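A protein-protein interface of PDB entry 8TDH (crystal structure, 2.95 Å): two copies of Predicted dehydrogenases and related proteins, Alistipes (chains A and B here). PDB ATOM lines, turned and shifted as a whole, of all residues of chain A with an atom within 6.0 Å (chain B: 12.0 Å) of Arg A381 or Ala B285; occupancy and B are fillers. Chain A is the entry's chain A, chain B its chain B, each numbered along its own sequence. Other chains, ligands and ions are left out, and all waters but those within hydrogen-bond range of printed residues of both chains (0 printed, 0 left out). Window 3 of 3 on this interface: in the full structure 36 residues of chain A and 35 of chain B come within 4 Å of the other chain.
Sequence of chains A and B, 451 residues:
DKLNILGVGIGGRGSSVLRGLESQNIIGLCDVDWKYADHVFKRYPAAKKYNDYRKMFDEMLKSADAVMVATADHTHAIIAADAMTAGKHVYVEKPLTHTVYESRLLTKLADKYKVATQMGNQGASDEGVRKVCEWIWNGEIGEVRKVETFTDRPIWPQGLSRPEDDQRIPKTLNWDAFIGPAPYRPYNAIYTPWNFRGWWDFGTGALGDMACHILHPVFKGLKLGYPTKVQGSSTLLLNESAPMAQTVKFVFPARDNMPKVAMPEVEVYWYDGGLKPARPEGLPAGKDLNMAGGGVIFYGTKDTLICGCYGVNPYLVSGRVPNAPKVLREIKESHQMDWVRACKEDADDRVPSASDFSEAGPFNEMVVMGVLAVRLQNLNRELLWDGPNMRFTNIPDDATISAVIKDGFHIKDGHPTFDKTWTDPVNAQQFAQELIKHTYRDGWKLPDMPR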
ATOM      1  N   VAL A 230     -15.915  17.401 -25.991  1.00  0.00           N
ATOM      2  CA  VAL A 230     -15.640  17.204 -24.587  1.00  0.00           C
ATOM      3  C   VAL A 230     -15.484  15.730 -24.285  1.00  0.00           C
ATOM      4  O   VAL A 230     -16.096  14.878 -24.899  1.00  0.00           O
ATOM      5  CB  VAL A 230     -16.740  17.878 -23.772  1.00  0.00           C
ATOM      6  CG1 VAL A 230     -18.093  17.260 -24.025  1.00  0.00           C
ATOM      7  CG2 VAL A 230     -16.333  17.916 -22.319  1.00  0.00           C
ATOM      8  N   GLN A 231     -14.570  15.474 -23.372  1.00  0.00           N
ATOM      9  CA  GLN A 231     -14.349  14.130 -22.862  1.00  0.00           C
ATOM     10  C   GLN A 231     -13.951  14.156 -21.379  1.00  0.00           C
ATOM     11  O   GLN A 231     -13.383  15.106 -20.903  1.00  0.00           O
ATOM     12  CB  GLN A 231     -13.386  13.403 -23.786  1.00  0.00           C
ATOM     13  CG  GLN A 231     -11.954  13.858 -23.623  1.00  0.00           C
ATOM     14  CD  GLN A 231     -11.026  13.080 -24.534  1.00  0.00           C
ATOM     15  OE1 GLN A 231     -10.664  13.551 -25.605  1.00  0.00           O
ATOM     16  NE2 GLN A 231     -10.682  11.848 -24.211  1.00  0.00           N
ATOM     17  N   LEU A 376     -21.138  10.163 -19.535  1.00  0.00           N
ATOM     18  CA  LEU A 376     -21.177   9.467 -20.808  1.00  0.00           C
ATOM     19  C   LEU A 376     -19.814   8.843 -21.120  1.00  0.00           C
ATOM     20  O   LEU A 376     -19.577   8.332 -22.202  1.00  0.00           O
ATOM     21  CB  LEU A 376     -21.668  10.462 -21.850  1.00  0.00           C
ATOM     22  CG  LEU A 376     -23.110  10.907 -21.637  1.00  0.00           C
ATOM     23  CD1 LEU A 376     -23.481  12.154 -22.414  1.00  0.00           C
ATOM     24  CD2 LEU A 376     -23.971   9.722 -22.087  1.00  0.00           C
ATOM     25  N   GLN A 377     -18.939   8.788 -20.123  1.00  0.00           N
ATOM     26  CA  GLN A 377     -17.579   8.360 -20.339  1.00  0.00           C
ATOM     27  C   GLN A 377     -17.457   6.952 -20.887  1.00  0.00           C
ATOM     28  O   GLN A 377     -16.410   6.589 -21.362  1.00  0.00           O
ATOM     29  CB  GLN A 377     -16.795   8.473 -19.040  1.00  0.00           C
ATOM     30  CG  GLN A 377     -17.113   7.459 -17.937  1.00  0.00           C
ATOM     31  CD  GLN A 377     -16.124   7.624 -16.813  1.00  0.00           C
ATOM     32  OE1 GLN A 377     -14.963   7.205 -16.912  1.00  0.00           O
ATOM     33  NE2 GLN A 377     -16.529   8.359 -15.792  1.00  0.00           N
ATOM     34  N   LEU A 379     -18.957   5.513 -23.297  1.00  0.00           N
ATOM     35  CA  LEU A 379     -19.021   5.557 -24.759  1.00  0.00           C
ATOM     36  C   LEU A 379     -17.630   5.525 -25.419  1.00  0.00           C
ATOM     37  O   LEU A 379     -17.546   5.120 -26.574  1.00  0.00           O
ATOM     38  CB  LEU A 379     -19.839   6.778 -25.188  1.00  0.00           C
ATOM     39  CG  LEU A 379     -21.281   6.858 -24.665  1.00  0.00           C
ATOM     40  CD1 LEU A 379     -22.015   8.078 -25.194  1.00  0.00           C
ATOM     41  CD2 LEU A 379     -22.043   5.627 -25.010  1.00  0.00           C
ATOM     42  N   ASN A 380     -16.552   5.937 -24.750  1.00  0.00           N
ATOM     43  CA  ASN A 380     -15.190   5.722 -25.244  1.00  0.00           C
ATOM     44  C   ASN A 380     -14.919   6.447 -26.570  1.00  0.00           C
ATOM     45  O   ASN A 380     -14.539   5.844 -27.569  1.00  0.00           O
ATOM     46  CB  ASN A 380     -14.890   4.241 -25.397  1.00  0.00           C
ATOM     47  CG  ASN A 380     -14.683   3.553 -24.071  1.00  0.00           C
ATOM     48  OD1 ASN A 380     -14.794   4.149 -22.981  1.00  0.00           O
ATOM     49  ND2 ASN A 380     -14.334   2.280 -24.165  1.00  0.00           N
ATOM     50  N   ARG A 381     -15.071   7.777 -26.511  1.00  0.00           N
ATOM     51  CA  ARG A 381     -15.213   8.646 -27.659  1.00  0.00           C
ATOM     52  C   ARG A 381     -15.173  10.103 -27.208  1.00  0.00           C
ATOM     53  O   ARG A 381     -15.882  10.528 -26.281  1.00  0.00           O
ATOM     54  CB  ARG A 381     -16.509   8.348 -28.404  1.00  0.00           C
ATOM     55  CG  ARG A 381     -17.799   9.017 -27.965  1.00  0.00           C
ATOM     56  CD  ARG A 381     -18.913   8.588 -28.920  1.00  0.00           C
ATOM     57  NE  ARG A 381     -18.972   7.134 -29.175  1.00  0.00           N
ATOM     58  CZ  ARG A 381     -19.033   6.513 -30.372  1.00  0.00           C
ATOM     59  NH1 ARG A 381     -19.180   7.193 -31.481  1.00  0.00           N
ATOM     60  NH2 ARG A 381     -18.970   5.203 -30.431  1.00  0.00           N
ATOM     61  N   GLU A 382     -14.351  10.884 -27.923  1.00  0.00           N
ATOM     62  CA  GLU A 382     -14.512  12.321 -27.844  1.00  0.00           C
ATOM     63  C   GLU A 382     -15.962  12.628 -28.182  1.00  0.00           C
ATOM     64  O   GLU A 382     -16.488  12.067 -29.113  1.00  0.00           O
ATOM     65  CB  GLU A 382     -13.494  12.907 -28.800  1.00  0.00           C
ATOM     66  CG  GLU A 382     -12.827  14.180 -28.274  1.00  0.00           C
ATOM     67  CD  GLU A 382     -11.709  14.640 -29.232  1.00  0.00           C
ATOM     68  OE1 GLU A 382     -11.479  14.064 -30.409  1.00  0.00           O
ATOM     69  OE2 GLU A 382     -11.068  15.633 -28.716  1.00  0.00           O
ATOM     70  N   LEU A 383     -16.654  13.410 -27.382  1.00  0.00           N
ATOM     71  CA  LEU A 383     -18.051  13.660 -27.676  1.00  0.00           C
ATOM     72  C   LEU A 383     -18.127  14.954 -28.459  1.00  0.00           C
ATOM     73  O   LEU A 383     -17.638  15.958 -27.991  1.00  0.00           O
ATOM     74  CB  LEU A 383     -18.870  13.745 -26.386  1.00  0.00           C
ATOM     75  CG  LEU A 383     -19.125  12.382 -25.743  1.00  0.00           C
ATOM     76  CD1 LEU A 383     -19.132  12.421 -24.232  1.00  0.00           C
ATOM     77  CD2 LEU A 383     -20.480  11.911 -26.211  1.00  0.00           C
ATOM     78  N   ASN A 394     -22.567  12.598 -32.106  1.00  0.00           N
ATOM     79  CA  ASN A 394     -21.736  11.478 -32.470  1.00  0.00           C
ATOM     80  C   ASN A 394     -21.923  10.300 -31.538  1.00  0.00           C
ATOM     81  O   ASN A 394     -20.996   9.519 -31.337  1.00  0.00           O
ATOM     82  CB  ASN A 394     -20.317  11.963 -32.656  1.00  0.00           C
ATOM     83  CG  ASN A 394     -19.534  12.024 -31.396  1.00  0.00           C
ATOM     84  OD1 ASN A 394     -19.897  12.748 -30.464  1.00  0.00           O
ATOM     85  ND2 ASN A 394     -18.435  11.297 -31.400  1.00  0.00           N
ATOM     86  N   ILE A 395     -23.152  10.161 -31.030  1.00  0.00           N
ATOM     87  CA  ILE A 395     -23.507   9.015 -30.222  1.00  0.00           C
ATOM     88  C   ILE A 395     -24.291   8.063 -31.120  1.00  0.00           C
ATOM     89  O   ILE A 395     -25.313   8.465 -31.657  1.00  0.00           O
ATOM     90  CB  ILE A 395     -24.358   9.403 -29.010  1.00  0.00           C
ATOM     91  CG1 ILE A 395     -23.771  10.481 -28.135  1.00  0.00           C
ATOM     92  CG2 ILE A 395     -24.607   8.143 -28.209  1.00  0.00           C
ATOM     93  CD1 ILE A 395     -24.723  10.960 -27.060  1.00  0.00           C
ATOM     94  N   PRO A 396     -23.878   6.785 -31.265  1.00  0.00           N
ATOM     95  CA  PRO A 396     -24.625   5.841 -32.066  1.00  0.00           C
ATOM     96  C   PRO A 396     -26.027   5.635 -31.503  1.00  0.00           C
ATOM     97  O   PRO A 396     -26.214   5.707 -30.286  1.00  0.00           O
ATOM     98  CB  PRO A 396     -23.779   4.564 -31.998  1.00  0.00           C
ATOM     99  CG  PRO A 396     -22.440   4.980 -31.437  1.00  0.00           C
ATOM    100  CD  PRO A 396     -22.681   6.201 -30.660  1.00  0.00           C
ATOM    101  N   ALA A 399     -25.890   2.352 -29.143  1.00  0.00           N
ATOM    102  CA  ALA A 399     -25.047   2.333 -27.958  1.00  0.00           C
ATOM    103  C   ALA A 399     -25.891   2.594 -26.727  1.00  0.00           C
ATOM    104  O   ALA A 399     -26.936   3.253 -26.806  1.00  0.00           O
ATOM    105  CB  ALA A 399     -23.935   3.351 -28.034  1.00  0.00           C
ATOM    106  N   PHE B 150      -2.002   3.512 -18.542  1.00  0.00           N
ATOM    107  CA  PHE B 150      -2.979   3.433 -17.472  1.00  0.00           C
ATOM    108  C   PHE B 150      -3.441   2.006 -17.215  1.00  0.00           C
ATOM    109  O   PHE B 150      -3.396   1.165 -18.109  1.00  0.00           O
ATOM    110  CB  PHE B 150      -4.228   4.259 -17.772  1.00  0.00           C
ATOM    111  CG  PHE B 150      -5.169   3.650 -18.788  1.00  0.00           C
ATOM    112  CD1 PHE B 150      -4.821   3.627 -20.132  1.00  0.00           C
ATOM    113  CD2 PHE B 150      -6.388   3.129 -18.394  1.00  0.00           C
ATOM    114  CE1 PHE B 150      -5.684   3.073 -21.068  1.00  0.00           C
ATOM    115  CE2 PHE B 150      -7.250   2.579 -19.330  1.00  0.00           C
ATOM    116  CZ  PHE B 150      -6.893   2.538 -20.663  1.00  0.00           C
ATOM    117  N   LYS B 276      -8.174   8.221 -17.152  1.00  0.00           N
ATOM    118  CA  LYS B 276      -7.683   7.784 -18.453  1.00  0.00           C
ATOM    119  C   LYS B 276      -7.005   8.924 -19.208  1.00  0.00           C
ATOM    120  O   LYS B 276      -7.463  10.079 -19.192  1.00  0.00           O
ATOM    121  CB  LYS B 276      -8.819   7.260 -19.344  1.00  0.00           C
ATOM    122  CG  LYS B 276      -9.138   5.783 -19.161  1.00  0.00           C
ATOM    123  CD  LYS B 276     -10.384   5.330 -19.892  1.00  0.00           C
ATOM    124  CE  LYS B 276     -11.279   6.502 -19.912  1.00  0.00           C
ATOM    125  NZ  LYS B 276     -12.594   6.061 -20.361  1.00  0.00           N
ATOM    126  N   PRO B 277      -5.969   8.588 -20.014  1.00  0.00           N
ATOM    127  CA  PRO B 277      -5.343   9.576 -20.897  1.00  0.00           C
ATOM    128  C   PRO B 277      -6.421   9.990 -21.898  1.00  0.00           C
ATOM    129  O   PRO B 277      -7.307   9.174 -22.204  1.00  0.00           O
ATOM    130  CB  PRO B 277      -4.166   8.801 -21.550  1.00  0.00           C
ATOM    131  CG  PRO B 277      -4.520   7.316 -21.430  1.00  0.00           C
ATOM    132  CD  PRO B 277      -5.448   7.212 -20.219  1.00  0.00           C
ATOM    133  N   ALA B 278      -6.347  11.240 -22.394  1.00  0.00           N
ATOM    134  CA  ALA B 278      -7.233  11.699 -23.467  1.00  0.00           C
ATOM    135  C   ALA B 278      -7.032  10.841 -24.707  1.00  0.00           C
ATOM    136  O   ALA B 278      -5.958  10.281 -24.909  1.00  0.00           O
ATOM    137  CB  ALA B 278      -7.071  13.180 -23.767  1.00  0.00           C
ATOM    138  N   ARG B 279      -8.099  10.701 -25.498  1.00  0.00           N
ATOM    139  CA  ARG B 279      -8.071   9.783 -26.622  1.00  0.00           C
ATOM    140  C   ARG B 279      -7.097  10.313 -27.680  1.00  0.00           C
ATOM    141  O   ARG B 279      -7.117  11.518 -27.968  1.00  0.00           O
ATOM    142  CB  ARG B 279      -9.471   9.614 -27.228  1.00  0.00           C
ATOM    143  CG  ARG B 279     -10.473   8.872 -26.358  1.00  0.00           C
ATOM    144  CD  ARG B 279     -11.751   8.609 -27.110  1.00  0.00           C
ATOM    145  NE  ARG B 279     -11.581   7.507 -28.067  1.00  0.00           N
ATOM    146  CZ  ARG B 279     -11.446   6.251 -27.733  1.00  0.00           C
ATOM    147  NH1 ARG B 279     -11.316   5.895 -26.475  1.00  0.00           N
ATOM    148  NH2 ARG B 279     -11.423   5.334 -28.662  1.00  0.00           N
ATOM    149  N   PRO B 280      -6.238   9.448 -28.280  1.00  0.00           N
ATOM    150  CA  PRO B 280      -5.409   9.826 -29.430  1.00  0.00           C
ATOM    151  C   PRO B 280      -6.214  10.295 -30.635  1.00  0.00           C
ATOM    152  O   PRO B 280      -7.304   9.794 -30.870  1.00  0.00           O
ATOM    153  CB  PRO B 280      -4.693   8.509 -29.774  1.00  0.00           C
ATOM    154  CG  PRO B 280      -4.713   7.701 -28.507  1.00  0.00           C
ATOM    155  CD  PRO B 280      -6.036   8.043 -27.883  1.00  0.00           C
ATOM    156  N   GLU B 281      -5.623  11.211 -31.405  1.00  0.00           N
ATOM    157  CA  GLU B 281      -6.118  11.564 -32.723  1.00  0.00           C
ATOM    158  C   GLU B 281      -5.997  10.343 -33.645  1.00  0.00           C
ATOM    159  O   GLU B 281      -5.002   9.599 -33.646  1.00  0.00           O
ATOM    160  CB  GLU B 281      -5.397  12.825 -33.208  1.00  0.00           C
ATOM    161  CG  GLU B 281      -5.675  13.151 -34.675  1.00  0.00           C
ATOM    162  CD  GLU B 281      -4.893  14.339 -35.256  1.00  0.00           C
ATOM    163  OE1 GLU B 281      -5.036  15.384 -34.545  1.00  0.00           O
ATOM    164  OE2 GLU B 281      -4.224  14.284 -36.361  1.00  0.00           O
ATOM    165  N   GLY B 282      -7.087  10.108 -34.376  1.00  0.00           N
ATOM    166  CA  GLY B 282      -7.105   9.059 -35.366  1.00  0.00           C
ATOM    167  C   GLY B 282      -7.841   7.811 -34.909  1.00  0.00           C
ATOM    168  O   GLY B 282      -8.342   7.065 -35.751  1.00  0.00           O
ATOM    169  N   LEU B 283      -7.873   7.562 -33.590  1.00  0.00           N
ATOM    170  CA  LEU B 283      -8.409   6.318 -33.057  1.00  0.00           C
ATOM    171  C   LEU B 283      -9.925   6.333 -33.195  1.00  0.00           C
ATOM    172  O   LEU B 283     -10.575   7.309 -32.840  1.00  0.00           O
ATOM    173  CB  LEU B 283      -7.984   6.174 -31.603  1.00  0.00           C
ATOM    174  CG  LEU B 283      -8.255   4.826 -30.918  1.00  0.00           C
ATOM    175  CD1 LEU B 283      -7.472   3.677 -31.531  1.00  0.00           C
ATOM    176  CD2 LEU B 283      -7.929   5.030 -29.437  1.00  0.00           C
ATOM    177  N   PRO B 284     -10.518   5.258 -33.756  1.00  0.00           N
ATOM    178  CA  PRO B 284     -11.976   5.133 -33.876  1.00  0.00           C
ATOM    179  C   PRO B 284     -12.778   5.434 -32.605  1.00  0.00           C
ATOM    180  O   PRO B 284     -12.472   4.967 -31.534  1.00  0.00           O
ATOM    181  CB  PRO B 284     -12.144   3.663 -34.309  1.00  0.00           C
ATOM    182  CG  PRO B 284     -10.894   3.384 -35.093  1.00  0.00           C
ATOM    183  CD  PRO B 284      -9.798   4.125 -34.366  1.00  0.00           C
ATOM    184  N   ALA B 285     -13.840   6.220 -32.748  1.00  0.00           N
ATOM    185  CA  ALA B 285     -14.829   6.374 -31.712  1.00  0.00           C
ATOM    186  C   ALA B 285     -15.335   4.988 -31.335  1.00  0.00           C
ATOM    187  O   ALA B 285     -15.638   4.171 -32.204  1.00  0.00           O
ATOM    188  CB  ALA B 285     -15.956   7.260 -32.200  1.00  0.00           C
ATOM    189  N   GLY B 286     -15.380   4.746 -30.009  1.00  0.00           N
ATOM    190  CA  GLY B 286     -15.883   3.512 -29.437  1.00  0.00           C
ATOM    191  C   GLY B 286     -14.759   2.550 -29.053  1.00  0.00           C
ATOM    192  O   GLY B 286     -14.961   1.673 -28.231  1.00  0.00           O
ATOM    193  N   LYS B 287     -13.589   2.634 -29.674  1.00  0.00           N
ATOM    194  CA  LYS B 287     -12.572   1.619 -29.466  1.00  0.00           C
ATOM    195  C   LYS B 287     -11.992   1.808 -28.078  1.00  0.00           C
ATOM    196  O   LYS B 287     -11.647   2.937 -27.711  1.00  0.00           O
ATOM    197  CB  LYS B 287     -11.493   1.742 -30.551  1.00  0.00           C
ATOM    198  CG  LYS B 287     -10.250   0.914 -30.420  1.00  0.00           C
ATOM    199  CD  LYS B 287     -10.422  -0.414 -31.143  1.00  0.00           C
ATOM    200  CE  LYS B 287      -9.271  -1.365 -30.912  1.00  0.00           C
ATOM    201  NZ  LYS B 287      -8.917  -1.440 -29.472  1.00  0.00           N
ATOM    202  N   ASP B 288     -11.909   0.702 -27.318  1.00  0.00           N
ATOM    203  CA  ASP B 288     -11.577   0.744 -25.899  1.00  0.00           C
ATOM    204  C   ASP B 288     -10.064   0.741 -25.751  1.00  0.00           C
ATOM    205  O   ASP B 288      -9.381  -0.097 -26.326  1.00  0.00           O
ATOM    206  CB  ASP B 288     -12.222  -0.395 -25.122  1.00  0.00           C
ATOM    207  CG  ASP B 288     -12.171  -0.372 -23.579  1.00  0.00           C
ATOM    208  OD1 ASP B 288     -11.412   0.454 -22.977  1.00  0.00           O
ATOM    209  OD2 ASP B 288     -12.914  -1.184 -22.927  1.00  0.00           O
ATOM    210  N   LEU B 289      -9.559   1.695 -24.965  1.00  0.00           N
ATOM    211  CA  LEU B 289      -8.141   1.811 -24.695  1.00  0.00           C
ATOM    212  C   LEU B 289      -7.667   0.688 -23.768  1.00  0.00           C
ATOM    213  O   LEU B 289      -6.488   0.298 -23.817  1.00  0.00           O
ATOM    214  CB  LEU B 289      -7.886   3.202 -24.126  1.00  0.00           C
ATOM    215  CG  LEU B 289      -7.955   4.365 -25.122  1.00  0.00           C
ATOM    216  CD1 LEU B 289      -7.668   5.717 -24.488  1.00  0.00           C
ATOM    217  CD2 LEU B 289      -6.939   4.144 -26.226  1.00  0.00           C
ATOM    218  N   ASN B 290      -8.596   0.167 -22.936  1.00  0.00           N
ATOM    219  CA  ASN B 290      -8.300  -0.890 -21.980  1.00  0.00           C
ATOM    220  C   ASN B 290      -8.320  -2.219 -22.717  1.00  0.00           C
ATOM    221  O   ASN B 290      -9.276  -2.517 -23.401  1.00  0.00           O
ATOM    222  CB  ASN B 290      -9.302  -0.934 -20.830  1.00  0.00           C
ATOM    223  CG  ASN B 290      -8.917  -1.962 -19.788  1.00  0.00           C
ATOM    224  OD1 ASN B 290      -8.474  -3.058 -20.162  1.00  0.00           O
ATOM    225  ND2 ASN B 290      -9.026  -1.629 -18.498  1.00  0.00           N
ATOM    226  N   ILE B 297      -0.201   4.077 -24.930  1.00  0.00           N
ATOM    227  CA  ILE B 297      -0.226   4.852 -26.161  1.00  0.00           C
ATOM    228  C   ILE B 297       1.170   5.439 -26.396  1.00  0.00           C
ATOM    229  O   ILE B 297       1.535   6.364 -25.684  1.00  0.00           O
ATOM    230  CB  ILE B 297      -1.319   5.939 -26.092  1.00  0.00           C
ATOM    231  CG1 ILE B 297      -2.688   5.339 -25.849  1.00  0.00           C
ATOM    232  CG2 ILE B 297      -1.339   6.819 -27.346  1.00  0.00           C
ATOM    233  CD1 ILE B 297      -3.681   6.312 -25.257  1.00  0.00           C
ATOM    234  N   ILE B 306      -0.494   1.530 -30.154  1.00  0.00           N
ATOM    235  CA  ILE B 306      -1.299   1.269 -28.966  1.00  0.00           C
ATOM    236  C   ILE B 306      -1.244  -0.218 -28.648  1.00  0.00           C
ATOM    237  O   ILE B 306      -1.397  -1.058 -29.519  1.00  0.00           O
ATOM    238  CB  ILE B 306      -2.754   1.728 -29.159  1.00  0.00           C
ATOM    239  CG1 ILE B 306      -2.863   3.203 -29.389  1.00  0.00           C
ATOM    240  CG2 ILE B 306      -3.589   1.358 -27.960  1.00  0.00           C
ATOM    241  CD1 ILE B 306      -4.229   3.678 -29.868  1.00  0.00           C
ATOM    242  N   TYR B 315      -1.241  -2.429 -32.138  1.00  0.00           N
ATOM    243  CA  TYR B 315      -1.762  -1.997 -33.418  1.00  0.00           C
ATOM    244  C   TYR B 315      -1.380  -0.538 -33.642  1.00  0.00           C
ATOM    245  O   TYR B 315      -1.156   0.189 -32.687  1.00  0.00           O
ATOM    246  CB  TYR B 315      -3.272  -2.236 -33.444  1.00  0.00           C
ATOM    247  CG  TYR B 315      -4.120  -1.425 -32.484  1.00  0.00           C
ATOM    248  CD1 TYR B 315      -4.302  -1.833 -31.175  1.00  0.00           C
ATOM    249  CD2 TYR B 315      -4.770  -0.272 -32.896  1.00  0.00           C
ATOM    250  CE1 TYR B 315      -5.031  -1.068 -30.275  1.00  0.00           C
ATOM    251  CE2 TYR B 315      -5.568   0.457 -32.023  1.00  0.00           C
ATOM    252  CZ  TYR B 315      -5.676   0.071 -30.695  1.00  0.00           C
ATOM    253  OH  TYR B 315      -6.412   0.741 -29.753  1.00  0.00           O
ATOM    254  N   VAL B 317      -2.512   3.207 -35.126  1.00  0.00           N
ATOM    255  CA  VAL B 317      -3.730   3.964 -35.370  1.00  0.00           C
ATOM    256  C   VAL B 317      -3.995   4.107 -36.858  1.00  0.00           C
ATOM    257  O   VAL B 317      -5.131   4.165 -37.280  1.00  0.00           O
ATOM    258  CB  VAL B 317      -3.657   5.344 -34.711  1.00  0.00           C
ATOM    259  CG1 VAL B 317      -4.798   6.238 -35.147  1.00  0.00           C
ATOM    260  CG2 VAL B 317      -3.662   5.183 -33.203  1.00  0.00           C
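NE2 of Gln A231 lies close to N of Arg B279 (3.1 Å). The backbone carbonyl oxygen of Asn A380 lies close to the guanidinium group of Arg B279 (3.3 Å). The backbone carbonyl oxygen (O) of Asn A380 lies within hydrogen-bond range of the backbone NH (N) of Gly B286, at 2.8 Å.
O of Gln A377 lies close to OD1 of Asn A380, at 3.3 Å. The backbone carbonyl oxygen (O) of Asn A394 is in hydrogen-bond range of the guanidinium group (NH1) of Arg A381 (3.0 Å). The backbone carbonyl oxygen of Glu A382 lies within hydrogen-bond range of the side-chain amide nitrogen of Asn A394 (3.1 Å). The backbone carbonyl oxygen of Lys B287 sits at hydrogen-bond distance from the guanidinium group of Arg B279 (2.6 Å). The side-chain amino group (NZ) of Lys B287 sits at hydrogen-bond distance from the side-chain hydroxyl (OH) of Tyr B315, at 3.3 Å. OD1 of Asp B288 sits at hydrogen-bond distance from N of Asn B290, at 2.8 Å.
Among the printed residues, merely in contact across the chains: Arg A381 with Ala B285 (3.3 Å), Asn A380 with Asp B288 (3.5 Å), Arg A381 with Arg B279 (3.5 Å), Gln A231 with Ala B278 (3.5 Å), Glu A382 with Arg B279 (3.5 Å), Arg A381 with Gly B286 (3.6 Å), Leu A379 with Gly B286 (3.7 Å), Asn A380 with Lys B276 (3.9 Å), Asn A380 with Ala B285 (3.9 Å), Asn A380 with Lys B287 (3.95 Å) and Gln A377 with Lys B276 (3.98 Å).
Gln A231 touches just these residues of chain B: Ala B278 and Arg B279. Leu A379 touches just one residue of chain B: Gly B286. Asn A380 touches just these residues of chain B: Lys B276, Arg B279, Ala B285, Gly B286, Lys B287 and Asp B288. Glu A382 touches one residue of chain B. No residue of chain B comes within 4 Å of Leu A383. No residue of chain B comes within 4 Å of Asn A394. No residue of chain B comes within 4 Å of Ile A395. No residue of chain B comes within 4 Å of Pro A396. Of the printed residues of chain A, Lys B276 touches Gln A377 (3.98 Å) and Asn A380 (3.9 Å). Of chain A, only Asn A380 (3.9 Å) and Arg A381 (3.3 Å) come within 4 Å of Ala B285. Printed residues of chain A within 4 Å of Gly B286: Leu A379 (3.7 Å), Asn A380 (2.8 Å) and Arg A381 (3.6 Å). Printed residues of chain A within 4 Å of Lys B287: Asn A380. Ile B297 touches none of the printed residues of chain A. The nearest residue of chain A that does not touch Ala B285 is Asn A394 (4.8 Å).
Along chain A the printed residues that touch a printed residue of chain B span positions 231 to 382. Hydrophobic or aromatic side chains of chain B within 4 Å of the printed part of chain A: Ala B278 and Ala B285. Among the printed residues, 14 pairs touch across the chains. Among the printed residues, no Asp or Glu carboxylate lies within 4 Å of a Lys or Arg side-chain nitrogen of the other chain.
No position is printed for both chains.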
